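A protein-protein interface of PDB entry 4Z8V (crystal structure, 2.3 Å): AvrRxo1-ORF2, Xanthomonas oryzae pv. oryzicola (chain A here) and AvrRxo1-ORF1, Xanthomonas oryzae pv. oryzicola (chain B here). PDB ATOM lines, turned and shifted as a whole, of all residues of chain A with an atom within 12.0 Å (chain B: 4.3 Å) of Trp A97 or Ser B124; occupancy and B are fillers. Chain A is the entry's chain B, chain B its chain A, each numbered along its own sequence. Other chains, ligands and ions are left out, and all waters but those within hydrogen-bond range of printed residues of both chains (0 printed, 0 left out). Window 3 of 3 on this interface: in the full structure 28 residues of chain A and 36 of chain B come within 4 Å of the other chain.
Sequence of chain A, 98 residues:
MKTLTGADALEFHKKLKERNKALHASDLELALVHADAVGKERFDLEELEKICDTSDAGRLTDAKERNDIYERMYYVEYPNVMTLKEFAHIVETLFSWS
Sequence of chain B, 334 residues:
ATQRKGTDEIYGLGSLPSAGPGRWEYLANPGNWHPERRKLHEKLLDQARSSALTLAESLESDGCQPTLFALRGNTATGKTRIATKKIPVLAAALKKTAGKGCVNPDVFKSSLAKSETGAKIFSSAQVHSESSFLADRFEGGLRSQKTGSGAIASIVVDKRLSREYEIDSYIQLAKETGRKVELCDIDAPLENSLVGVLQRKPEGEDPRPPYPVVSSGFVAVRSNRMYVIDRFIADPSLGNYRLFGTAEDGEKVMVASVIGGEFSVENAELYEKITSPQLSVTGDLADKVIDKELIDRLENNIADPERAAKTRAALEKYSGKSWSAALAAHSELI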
ATOM      1  N   ASP A  53      23.055  10.692  24.856  1.00  0.00           N
ATOM      2  CA  ASP A  53      23.168  12.138  24.716  1.00  0.00           C
ATOM      3  C   ASP A  53      21.876  12.852  25.116  1.00  0.00           C
ATOM      4  O   ASP A  53      20.790  12.527  24.620  1.00  0.00           O
ATOM      5  CB  ASP A  53      23.558  12.499  23.278  1.00  0.00           C
ATOM      6  CG  ASP A  53      23.598  13.999  23.040  1.00  0.00           C
ATOM      7  OD1 ASP A  53      23.996  14.749  23.959  1.00  0.00           O
ATOM      8  OD2 ASP A  53      23.224  14.427  21.927  1.00  0.00           O
ATOM      9  N   SER A  55      22.019  16.433  25.455  1.00  0.00           N
ATOM     10  CA  SER A  55      22.033  17.660  24.683  1.00  0.00           C
ATOM     11  C   SER A  55      21.292  17.329  23.392  1.00  0.00           C
ATOM     12  O   SER A  55      21.322  16.184  22.932  1.00  0.00           O
ATOM     13  CB  SER A  55      23.469  18.089  24.387  1.00  0.00           C
ATOM     14  OG  SER A  55      24.185  17.062  23.721  1.00  0.00           O
ATOM     15  N   ASP A  56      20.597  18.303  22.823  1.00  0.00           N
ATOM     16  CA  ASP A  56      19.939  18.080  21.539  1.00  0.00           C
ATOM     17  C   ASP A  56      20.937  18.449  20.447  1.00  0.00           C
ATOM     18  O   ASP A  56      20.727  19.401  19.693  1.00  0.00           O
ATOM     19  CB  ASP A  56      18.660  18.916  21.436  1.00  0.00           C
ATOM     20  CG  ASP A  56      17.830  18.580  20.203  1.00  0.00           C
ATOM     21  OD1 ASP A  56      18.130  17.570  19.522  1.00  0.00           O
ATOM     22  OD2 ASP A  56      16.868  19.331  19.924  1.00  0.00           O
ATOM     23  N   ALA A  57      22.020  17.674  20.375  1.00  0.00           N
ATOM     24  CA  ALA A  57      23.221  18.051  19.629  1.00  0.00           C
ATOM     25  C   ALA A  57      23.634  19.479  19.980  1.00  0.00           C
ATOM     26  O   ALA A  57      23.872  20.307  19.102  1.00  0.00           O
ATOM     27  CB  ALA A  57      23.019  17.890  18.125  1.00  0.00           C
ATOM     28  N   ARG A  59      21.896  21.825  21.141  1.00  0.00           N
ATOM     29  CA  ARG A  59      20.802  22.791  21.128  1.00  0.00           C
ATOM     30  C   ARG A  59      20.338  23.009  22.561  1.00  0.00           C
ATOM     31  O   ARG A  59      19.963  24.123  22.946  1.00  0.00           O
ATOM     32  CB  ARG A  59      19.641  22.335  20.227  1.00  0.00           C
ATOM     33  CG  ARG A  59      18.802  23.500  19.679  1.00  0.00           C
ATOM     34  CD  ARG A  59      17.481  23.068  19.036  1.00  0.00           C
ATOM     35  NE  ARG A  59      16.712  24.236  18.603  1.00  0.00           N
ATOM     36  CZ  ARG A  59      16.855  24.828  17.419  1.00  0.00           C
ATOM     37  NH1 ARG A  59      17.731  24.357  16.537  1.00  0.00           N
ATOM     38  NH2 ARG A  59      16.122  25.893  17.111  1.00  0.00           N
ATOM     39  N   TYR A  70      14.610  15.468  31.856  1.00  0.00           N
ATOM     40  CA  TYR A  70      14.816  14.024  31.905  1.00  0.00           C
ATOM     41  C   TYR A  70      14.496  13.332  33.228  1.00  0.00           C
ATOM     42  O   TYR A  70      14.041  12.192  33.228  1.00  0.00           O
ATOM     43  CB  TYR A  70      16.225  13.672  31.430  1.00  0.00           C
ATOM     44  CG  TYR A  70      16.372  13.902  29.957  1.00  0.00           C
ATOM     45  CD1 TYR A  70      15.868  12.982  29.052  1.00  0.00           C
ATOM     46  CD2 TYR A  70      16.970  15.060  29.466  1.00  0.00           C
ATOM     47  CE1 TYR A  70      15.964  13.187  27.699  1.00  0.00           C
ATOM     48  CE2 TYR A  70      17.078  15.280  28.103  1.00  0.00           C
ATOM     49  CZ  TYR A  70      16.570  14.332  27.228  1.00  0.00           C
ATOM     50  OH  TYR A  70      16.661  14.505  25.869  1.00  0.00           O
ATOM     51  N   MET A  73      10.727  13.214  33.178  1.00  0.00           N
ATOM     52  CA  MET A  73      10.303  12.209  32.201  1.00  0.00           C
ATOM     53  C   MET A  73      10.502  10.786  32.742  1.00  0.00           C
ATOM     54  O   MET A  73       9.632   9.927  32.606  1.00  0.00           O
ATOM     55  CB  MET A  73      11.078  12.389  30.891  1.00  0.00           C
ATOM     56  CG  MET A  73      10.773  11.347  29.850  1.00  0.00           C
ATOM     57  SD  MET A  73      11.824  11.447  28.377  1.00  0.00           S
ATOM     58  CE  MET A  73      11.478  13.110  27.810  1.00  0.00           C
ATOM     59  N   TYR A  78       7.503   7.354  32.695  1.00  0.00           N
ATOM     60  CA  TYR A  78       7.959   6.003  32.538  1.00  0.00           C
ATOM     61  C   TYR A  78       8.119   5.296  33.843  1.00  0.00           C
ATOM     62  O   TYR A  78       9.166   4.829  34.157  1.00  0.00           O
ATOM     63  CB  TYR A  78       9.256   6.000  31.741  1.00  0.00           C
ATOM     64  CG  TYR A  78       9.053   6.487  30.333  1.00  0.00           C
ATOM     65  CD1 TYR A  78       8.501   5.676  29.385  1.00  0.00           C
ATOM     66  CD2 TYR A  78       9.348   7.760  29.986  1.00  0.00           C
ATOM     67  CE1 TYR A  78       8.289   6.100  28.156  1.00  0.00           C
ATOM     68  CE2 TYR A  78       9.146   8.187  28.758  1.00  0.00           C
ATOM     69  CZ  TYR A  78       8.613   7.357  27.834  1.00  0.00           C
ATOM     70  OH  TYR A  78       8.388   7.783  26.593  1.00  0.00           O
ATOM     71  N   ALA A  88      17.710   4.852  28.979  1.00  0.00           N
ATOM     72  CA  ALA A  88      18.595   5.281  27.929  1.00  0.00           C
ATOM     73  C   ALA A  88      18.130   4.807  26.569  1.00  0.00           C
ATOM     74  O   ALA A  88      18.284   5.491  25.618  1.00  0.00           O
ATOM     75  CB  ALA A  88      19.932   4.800  28.191  1.00  0.00           C
ATOM     76  N   HIS A  89      17.559   3.625  26.506  1.00  0.00           N
ATOM     77  CA  HIS A  89      17.028   3.099  25.288  1.00  0.00           C
ATOM     78  C   HIS A  89      15.957   4.009  24.816  1.00  0.00           C
ATOM     79  O   HIS A  89      15.831   4.261  23.660  1.00  0.00           O
ATOM     80  CB  HIS A  89      16.340   1.775  25.525  1.00  0.00           C
ATOM     81  CG  HIS A  89      17.243   0.668  25.943  1.00  0.00           C
ATOM     82  ND1 HIS A  89      18.598   0.677  25.706  1.00  0.00           N
ATOM     83  CD2 HIS A  89      16.974  -0.498  26.575  1.00  0.00           C
ATOM     84  CE1 HIS A  89      19.127  -0.434  26.178  1.00  0.00           C
ATOM     85  NE2 HIS A  89      18.163  -1.163  26.709  1.00  0.00           N
ATOM     86  N   ILE A  90      15.152   4.463  25.742  1.00  0.00           N
ATOM     87  CA  ILE A  90      14.067   5.355  25.466  1.00  0.00           C
ATOM     88  C   ILE A  90      14.548   6.694  24.988  1.00  0.00           C
ATOM     89  O   ILE A  90      14.048   7.221  24.042  1.00  0.00           O
ATOM     90  CB  ILE A  90      13.222   5.561  26.700  1.00  0.00           C
ATOM     91  CG1 ILE A  90      12.557   4.282  27.063  1.00  0.00           C
ATOM     92  CG2 ILE A  90      12.154   6.538  26.458  1.00  0.00           C
ATOM     93  CD1 ILE A  90      11.352   4.497  27.733  1.00  0.00           C
ATOM     94  N   VAL A  91      15.520   7.248  25.664  1.00  0.00           N
ATOM     95  CA  VAL A  91      15.987   8.546  25.291  1.00  0.00           C
ATOM     96  C   VAL A  91      16.603   8.526  23.909  1.00  0.00           C
ATOM     97  O   VAL A  91      16.423   9.428  23.156  1.00  0.00           O
ATOM     98  CB  VAL A  91      16.947   9.078  26.326  1.00  0.00           C
ATOM     99  CG1 VAL A  91      17.589  10.296  25.848  1.00  0.00           C
ATOM    100  CG2 VAL A  91      16.215   9.368  27.579  1.00  0.00           C
ATOM    101  N   GLU A  92      17.333   7.470  23.615  1.00  0.00           N
ATOM    102  CA  GLU A  92      17.928   7.253  22.296  1.00  0.00           C
ATOM    103  C   GLU A  92      16.857   7.176  21.220  1.00  0.00           C
ATOM    104  O   GLU A  92      17.038   7.677  20.111  1.00  0.00           O
ATOM    105  CB  GLU A  92      18.762   5.962  22.287  1.00  0.00           C
ATOM    106  CG  GLU A  92      20.156   6.093  22.940  1.00  0.00           C
ATOM    107  CD  GLU A  92      20.690   4.763  23.501  1.00  0.00           C
ATOM    108  OE1 GLU A  92      20.119   3.682  23.197  1.00  0.00           O
ATOM    109  OE2 GLU A  92      21.685   4.807  24.256  1.00  0.00           O
ATOM    110  N   THR A  93      15.744   6.534  21.559  1.00  0.00           N
ATOM    111  CA  THR A  93      14.603   6.435  20.662  1.00  0.00           C
ATOM    112  C   THR A  93      14.060   7.834  20.374  1.00  0.00           C
ATOM    113  O   THR A  93      13.793   8.182  19.223  1.00  0.00           O
ATOM    114  CB  THR A  93      13.514   5.558  21.293  1.00  0.00           C
ATOM    115  OG1 THR A  93      14.040   4.240  21.503  1.00  0.00           O
ATOM    116  CG2 THR A  93      12.274   5.488  20.410  1.00  0.00           C
ATOM    117  N   LEU A  94      13.928   8.645  21.418  1.00  0.00           N
ATOM    118  CA  LEU A  94      13.358   9.977  21.260  1.00  0.00           C
ATOM    119  C   LEU A  94      14.247  10.863  20.398  1.00  0.00           C
ATOM    120  O   LEU A  94      13.759  11.731  19.660  1.00  0.00           O
ATOM    121  CB  LEU A  94      13.158  10.641  22.616  1.00  0.00           C
ATOM    122  CG  LEU A  94      12.157  10.036  23.595  1.00  0.00           C
ATOM    123  CD1 LEU A  94      12.058  10.945  24.821  1.00  0.00           C
ATOM    124  CD2 LEU A  94      10.799   9.869  22.929  1.00  0.00           C
ATOM    125  N   PHE A  95      15.550  10.635  20.496  1.00  0.00           N
ATOM    126  CA  PHE A  95      16.525  11.452  19.790  1.00  0.00           C
ATOM    127  C   PHE A  95      16.636  11.057  18.314  1.00  0.00           C
ATOM    128  O   PHE A  95      17.011  11.875  17.481  1.00  0.00           O
ATOM    129  CB  PHE A  95      17.868  11.425  20.545  1.00  0.00           C
ATOM    130  CG  PHE A  95      19.040  10.989  19.718  1.00  0.00           C
ATOM    131  CD1 PHE A  95      19.265   9.635  19.459  1.00  0.00           C
ATOM    132  CD2 PHE A  95      19.938  11.930  19.224  1.00  0.00           C
ATOM    133  CE1 PHE A  95      20.347   9.234  18.698  1.00  0.00           C
ATOM    134  CE2 PHE A  95      21.026  11.541  18.469  1.00  0.00           C
ATOM    135  CZ  PHE A  95      21.232  10.190  18.201  1.00  0.00           C
ATOM    136  N   SER A  96      16.268   9.815  18.002  1.00  0.00           N
ATOM    137  CA  SER A  96      16.228   9.315  16.626  1.00  0.00           C
ATOM    138  C   SER A  96      15.038   9.829  15.821  1.00  0.00           C
ATOM    139  O   SER A  96      14.948   9.589  14.614  1.00  0.00           O
ATOM    140  CB  SER A  96      16.182   7.788  16.624  1.00  0.00           C
ATOM    141  OG  SER A  96      17.395   7.235  17.088  1.00  0.00           O
ATOM    142  N   TRP A  97      14.109  10.513  16.479  1.00  0.00           N
ATOM    143  CA  TRP A  97      12.943  11.024  15.772  1.00  0.00           C
ATOM    144  C   TRP A  97      12.759  12.518  15.994  1.00  0.00           C
ATOM    145  O   TRP A  97      13.423  13.126  16.844  1.00  0.00           O
ATOM    146  CB  TRP A  97      11.688  10.264  16.196  1.00  0.00           C
ATOM    147  CG  TRP A  97      11.753   8.844  15.788  1.00  0.00           C
ATOM    148  CD1 TRP A  97      12.321   7.809  16.483  1.00  0.00           C
ATOM    149  CD2 TRP A  97      11.270   8.286  14.565  1.00  0.00           C
ATOM    150  NE1 TRP A  97      12.211   6.644  15.768  1.00  0.00           N
ATOM    151  CE2 TRP A  97      11.564   6.909  14.579  1.00  0.00           C
ATOM    152  CE3 TRP A  97      10.617   8.825  13.446  1.00  0.00           C
ATOM    153  CZ2 TRP A  97      11.228   6.052  13.522  1.00  0.00           C
ATOM    154  CZ3 TRP A  97      10.277   7.983  12.401  1.00  0.00           C
ATOM    155  CH2 TRP A  97      10.579   6.611  12.443  1.00  0.00           C
ATOM    156  N   SER A  98      11.871  13.105  15.199  1.00  0.00           N
ATOM    157  CA  SER A  98      11.474  14.491  15.371  1.00  0.00           C
ATOM    158  C   SER A  98      10.293  14.487  16.337  1.00  0.00           C
ATOM    159  O   SER A  98       9.440  13.587  16.281  1.00  0.00           O
ATOM    160  CB  SER A  98      11.040  15.099  14.030  1.00  0.00           C
ATOM    161  OG  SER A  98      12.075  15.057  13.055  1.00  0.00           O
ATOM    162  N   LYS B 109      14.626  13.646   4.866  1.00  0.00           N
ATOM    163  CA  LYS B 109      14.668  12.221   5.208  1.00  0.00           C
ATOM    164  C   LYS B 109      14.442  11.253   4.048  1.00  0.00           C
ATOM    165  O   LYS B 109      15.163  10.272   3.918  1.00  0.00           O
ATOM    166  CB  LYS B 109      13.674  11.893   6.333  1.00  0.00           C
ATOM    167  CG  LYS B 109      14.074  12.406   7.713  1.00  0.00           C
ATOM    168  CD  LYS B 109      14.088  11.266   8.722  1.00  0.00           C
ATOM    169  CE  LYS B 109      13.546  11.697  10.073  1.00  0.00           C
ATOM    170  NZ  LYS B 109      14.093  13.011  10.493  1.00  0.00           N
ATOM    171  N   PHE B 122      17.466   3.176   3.534  1.00  0.00           N
ATOM    172  CA  PHE B 122      17.814   3.448   4.927  1.00  0.00           C
ATOM    173  C   PHE B 122      16.529   3.700   5.718  1.00  0.00           C
ATOM    174  O   PHE B 122      15.575   4.246   5.185  1.00  0.00           O
ATOM    175  CB  PHE B 122      18.737   4.660   5.019  1.00  0.00           C
ATOM    176  CG  PHE B 122      20.082   4.460   4.373  1.00  0.00           C
ATOM    177  CD1 PHE B 122      20.890   3.381   4.716  1.00  0.00           C
ATOM    178  CD2 PHE B 122      20.546   5.369   3.424  1.00  0.00           C
ATOM    179  CE1 PHE B 122      22.139   3.196   4.112  1.00  0.00           C
ATOM    180  CE2 PHE B 122      21.787   5.196   2.808  1.00  0.00           C
ATOM    181  CZ  PHE B 122      22.589   4.106   3.155  1.00  0.00           C
ATOM    182  N   SER B 123      16.494   3.305   6.981  1.00  0.00           N
ATOM    183  CA  SER B 123      15.331   3.603   7.818  1.00  0.00           C
ATOM    184  C   SER B 123      15.373   5.069   8.242  1.00  0.00           C
ATOM    185  O   SER B 123      16.441   5.696   8.221  1.00  0.00           O
ATOM    186  CB  SER B 123      15.342   2.737   9.067  1.00  0.00           C
ATOM    187  OG  SER B 123      16.407   3.124   9.918  1.00  0.00           O
ATOM    188  N   SER B 124      14.218   5.613   8.620  1.00  0.00           N
ATOM    189  CA  SER B 124      14.141   6.980   9.119  1.00  0.00           C
ATOM    190  C   SER B 124      15.185   7.243  10.197  1.00  0.00           C
ATOM    191  O   SER B 124      15.846   8.288  10.198  1.00  0.00           O
ATOM    192  CB  SER B 124      12.740   7.270   9.667  1.00  0.00           C
ATOM    193  OG  SER B 124      11.888   7.707   8.632  1.00  0.00           O
ATOM    194  N   ALA B 125      15.359   6.282  11.095  1.00  0.00           N
ATOM    195  CA  ALA B 125      16.309   6.454  12.188  1.00  0.00           C
ATOM    196  C   ALA B 125      17.752   6.477  11.700  1.00  0.00           C
ATOM    197  O   ALA B 125      18.603   7.132  12.311  1.00  0.00           O
ATOM    198  CB  ALA B 125      16.121   5.378  13.225  1.00  0.00           C
ATOM    199  N   GLN B 126      18.030   5.752  10.617  1.00  0.00           N
ATOM    200  CA  GLN B 126      19.366   5.745  10.032  1.00  0.00           C
ATOM    201  C   GLN B 126      19.731   7.113   9.468  1.00  0.00           C
ATOM    202  O   GLN B 126      20.878   7.559   9.615  1.00  0.00           O
ATOM    203  CB  GLN B 126      19.476   4.684   8.932  1.00  0.00           C
ATOM    204  CG  GLN B 126      19.564   3.255   9.439  1.00  0.00           C
ATOM    205  CD  GLN B 126      19.908   2.279   8.336  1.00  0.00           C
ATOM    206  OE1 GLN B 126      19.041   1.870   7.556  1.00  0.00           O
ATOM    207  NE2 GLN B 126      21.183   1.908   8.254  1.00  0.00           N
ATOM    208  N   VAL B 127      18.758   7.773   8.835  1.00  0.00           N
ATOM    209  CA  VAL B 127      18.997   9.085   8.236  1.00  0.00           C
ATOM    210  C   VAL B 127      18.691  10.284   9.144  1.00  0.00           C
ATOM    211  O   VAL B 127      18.866  11.422   8.710  1.00  0.00           O
ATOM    212  CB  VAL B 127      18.190   9.301   6.929  1.00  0.00           C
ATOM    213  CG1 VAL B 127      18.437   8.199   5.936  1.00  0.00           C
ATOM    214  CG2 VAL B 127      16.702   9.431   7.229  1.00  0.00           C
ATOM    215  N   HIS B 128      18.219  10.056  10.371  1.00  0.00           N
ATOM    216  CA  HIS B 128      17.713  11.181  11.172  1.00  0.00           C
ATOM    217  C   HIS B 128      18.794  12.204  11.517  1.00  0.00           C
ATOM    218  O   HIS B 128      18.612  13.402  11.322  1.00  0.00           O
ATOM    219  CB  HIS B 128      17.014  10.746  12.465  1.00  0.00           C
ATOM    220  CG  HIS B 128      16.647  11.899  13.347  1.00  0.00           C
ATOM    221  ND1 HIS B 128      15.515  12.667  13.146  1.00  0.00           N
ATOM    222  CD2 HIS B 128      17.292  12.459  14.405  1.00  0.00           C
ATOM    223  CE1 HIS B 128      15.466  13.629  14.050  1.00  0.00           C
ATOM    224  NE2 HIS B 128      16.531  13.524  14.827  1.00  0.00           N
ATOM    225  N   ARG B 208       6.847   8.009  10.676  1.00  0.00           N
ATOM    226  CA  ARG B 208       6.147   7.014  11.432  1.00  0.00           C
ATOM    227  C   ARG B 208       6.863   6.666  12.704  1.00  0.00           C
ATOM    228  O   ARG B 208       7.464   5.668  12.807  1.00  0.00           O
ATOM    229  CB  ARG B 208       5.981   5.780  10.598  1.00  0.00           C
ATOM    230  CG  ARG B 208       4.891   5.867   9.626  1.00  0.00           C
ATOM    231  CD  ARG B 208       5.027   4.815   8.551  1.00  0.00           C
ATOM    232  NE  ARG B 208       6.241   4.960   7.792  1.00  0.00           N
ATOM    233  CZ  ARG B 208       7.172   4.044   7.715  1.00  0.00           C
ATOM    234  NH1 ARG B 208       7.033   2.916   8.340  1.00  0.00           N
ATOM    235  NH2 ARG B 208       8.241   4.257   7.019  1.00  0.00           N
ATOM    236  N   PRO B 209       6.791   7.517  13.688  1.00  0.00           N
ATOM    237  CA  PRO B 209       7.565   7.283  14.909  1.00  0.00           C
ATOM    238  C   PRO B 209       6.906   6.259  15.820  1.00  0.00           C
ATOM    239  O   PRO B 209       5.693   6.035  15.708  1.00  0.00           O
ATOM    240  CB  PRO B 209       7.582   8.670  15.579  1.00  0.00           C
ATOM    241  CG  PRO B 209       6.352   9.357  15.082  1.00  0.00           C
ATOM    242  CD  PRO B 209       6.107   8.828  13.695  1.00  0.00           C
ATOM    243  N   PRO B 210       7.697   5.631  16.715  1.00  0.00           N
ATOM    244  CA  PRO B 210       7.115   4.663  17.651  1.00  0.00           C
ATOM    245  C   PRO B 210       6.406   5.364  18.801  1.00  0.00           C
ATOM    246  O   PRO B 210       6.523   6.580  18.932  1.00  0.00           O
ATOM    247  CB  PRO B 210       8.343   3.910  18.178  1.00  0.00           C
ATOM    248  CG  PRO B 210       9.455   4.939  18.122  1.00  0.00           C
ATOM    249  CD  PRO B 210       9.159   5.767  16.883  1.00  0.00           C
ATOM    250  N   VAL B 213       7.831   8.383  21.260  1.00  0.00           N
ATOM    251  CA  VAL B 213       7.990   9.671  20.594  1.00  0.00           C
ATOM    252  C   VAL B 213       6.675  10.458  20.615  1.00  0.00           C
ATOM    253  O   VAL B 213       6.651  11.652  20.948  1.00  0.00           O
ATOM    254  CB  VAL B 213       8.473   9.479  19.154  1.00  0.00           C
ATOM    255  CG1 VAL B 213       8.389  10.797  18.357  1.00  0.00           C
ATOM    256  CG2 VAL B 213       9.882   8.939  19.167  1.00  0.00           C
ATOM    257  N   SER B 331       6.391   1.431  12.711  1.00  0.00           N
ATOM    258  CA  SER B 331       7.605   2.236  12.628  1.00  0.00           C
ATOM    259  C   SER B 331       8.762   1.540  11.902  1.00  0.00           C
ATOM    260  O   SER B 331       9.529   2.194  11.196  1.00  0.00           O
ATOM    261  CB  SER B 331       8.071   2.611  14.030  1.00  0.00           C
ATOM    262  OG  SER B 331       8.929   3.732  13.974  1.00  0.00           O
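Hydrophobic or aromatic side chains of chain B that line the printed part of chain A: His B128, Pro B209, Pro B210 and Val B213. Printed residues of chain A that touch a printed residue of chain B: Thr A93, Leu A94, Phe A95, Ser A96, Trp A97 and Ser A98. Hydrophobic or aromatic side chains of chain A within 4 Å of the printed part of chain B: Leu A94 and Trp A97. Among the printed residues, no Asp or Glu carboxylate lies within 4 Å of a Lys or Arg side-chain nitrogen of the other chain.
A ring nitrogen (NE2) of His B128 sits close to the backbone carbonyl oxygen of Phe A95 (3.2 Å). A ring nitrogen (ND1) of His B128 lies close to the backbone carbonyl oxygen of Ser A96, at 3.5 Å.
The side-chain amino group (NZ) of Lys B109 is in hydrogen-bond range of a ring nitrogen (ND1) of His B128. The side-chain hydroxyl of Ser B331 sits at hydrogen-bond distance from the backbone carbonyl oxygen of Arg B208, at 2.7 Å. OG1 of Thr A93 sits at hydrogen-bond distance from O of His A89 (2.8 Å). The side-chain hydroxyl (OG) of Ser A96 lies within hydrogen-bond range of the backbone carbonyl oxygen (O) of Glu A92 (3.1 Å).
Ser B124 touches one residue of chain A. Of the printed residues of chain A, Lys B109 touches Ser A98 (3.8 Å). Ala B125 touches none of the printed residues of chain A. Gln B126 touches none of the printed residues of chain A. No residue of chain A comes within 4 Å of Val B127. Of chain A, only Phe A95 (3.1 Å), Ser A96 (3.1 Å), Trp A97 (3.5 Å) and Ser A98 (3.8 Å) come within 4 Å of His B128. Of chain A, only Trp A97 comes within 4 Å of Arg B208. Pro B210 touches just these residues of chain A: Thr A93 and Trp A97. Printed residues of chain A within 4 Å of Ser B331: Trp A97 (3.3 Å). Printed residues of chain B within 4 Å of Leu A94: Val B213. Of the printed residues of chain B, Ser A96 touches His B128. Of the printed residues of chain B, Phe A95 touches His B128 (3.1 Å). Asp A56 touches none of the printed residues of chain B. Arg A59 touches none of the printed residues of chain B. The nearest printed residue of chain B that does not touch Leu A94 is His B128 (5.9 Å).
Among the printed residues, pairs that only touch across the chains: Trp A97 with Arg B208 (3.3 Å), Trp A97 with Ser B331 (3.3 Å), Trp A97 with Pro B210 (3.4 Å), Trp A97 with His B128 (3.5 Å), Trp A97 with Ser B124 (3.6 Å), Ser A98 with Val B213 (3.6 Å), Leu A94 with Val B213 (3.7 Å), Thr A93 with Pro B210 (3.7 Å), Trp A97 with Pro B209 (3.7 Å), Trp A97 with Val B213 (3.7 Å), Ser A98 with His B128 (3.8 Å), Ser A98 with Lys B109 (3.8 Å) and Thr A93 with Val B213 (3.98 Å).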
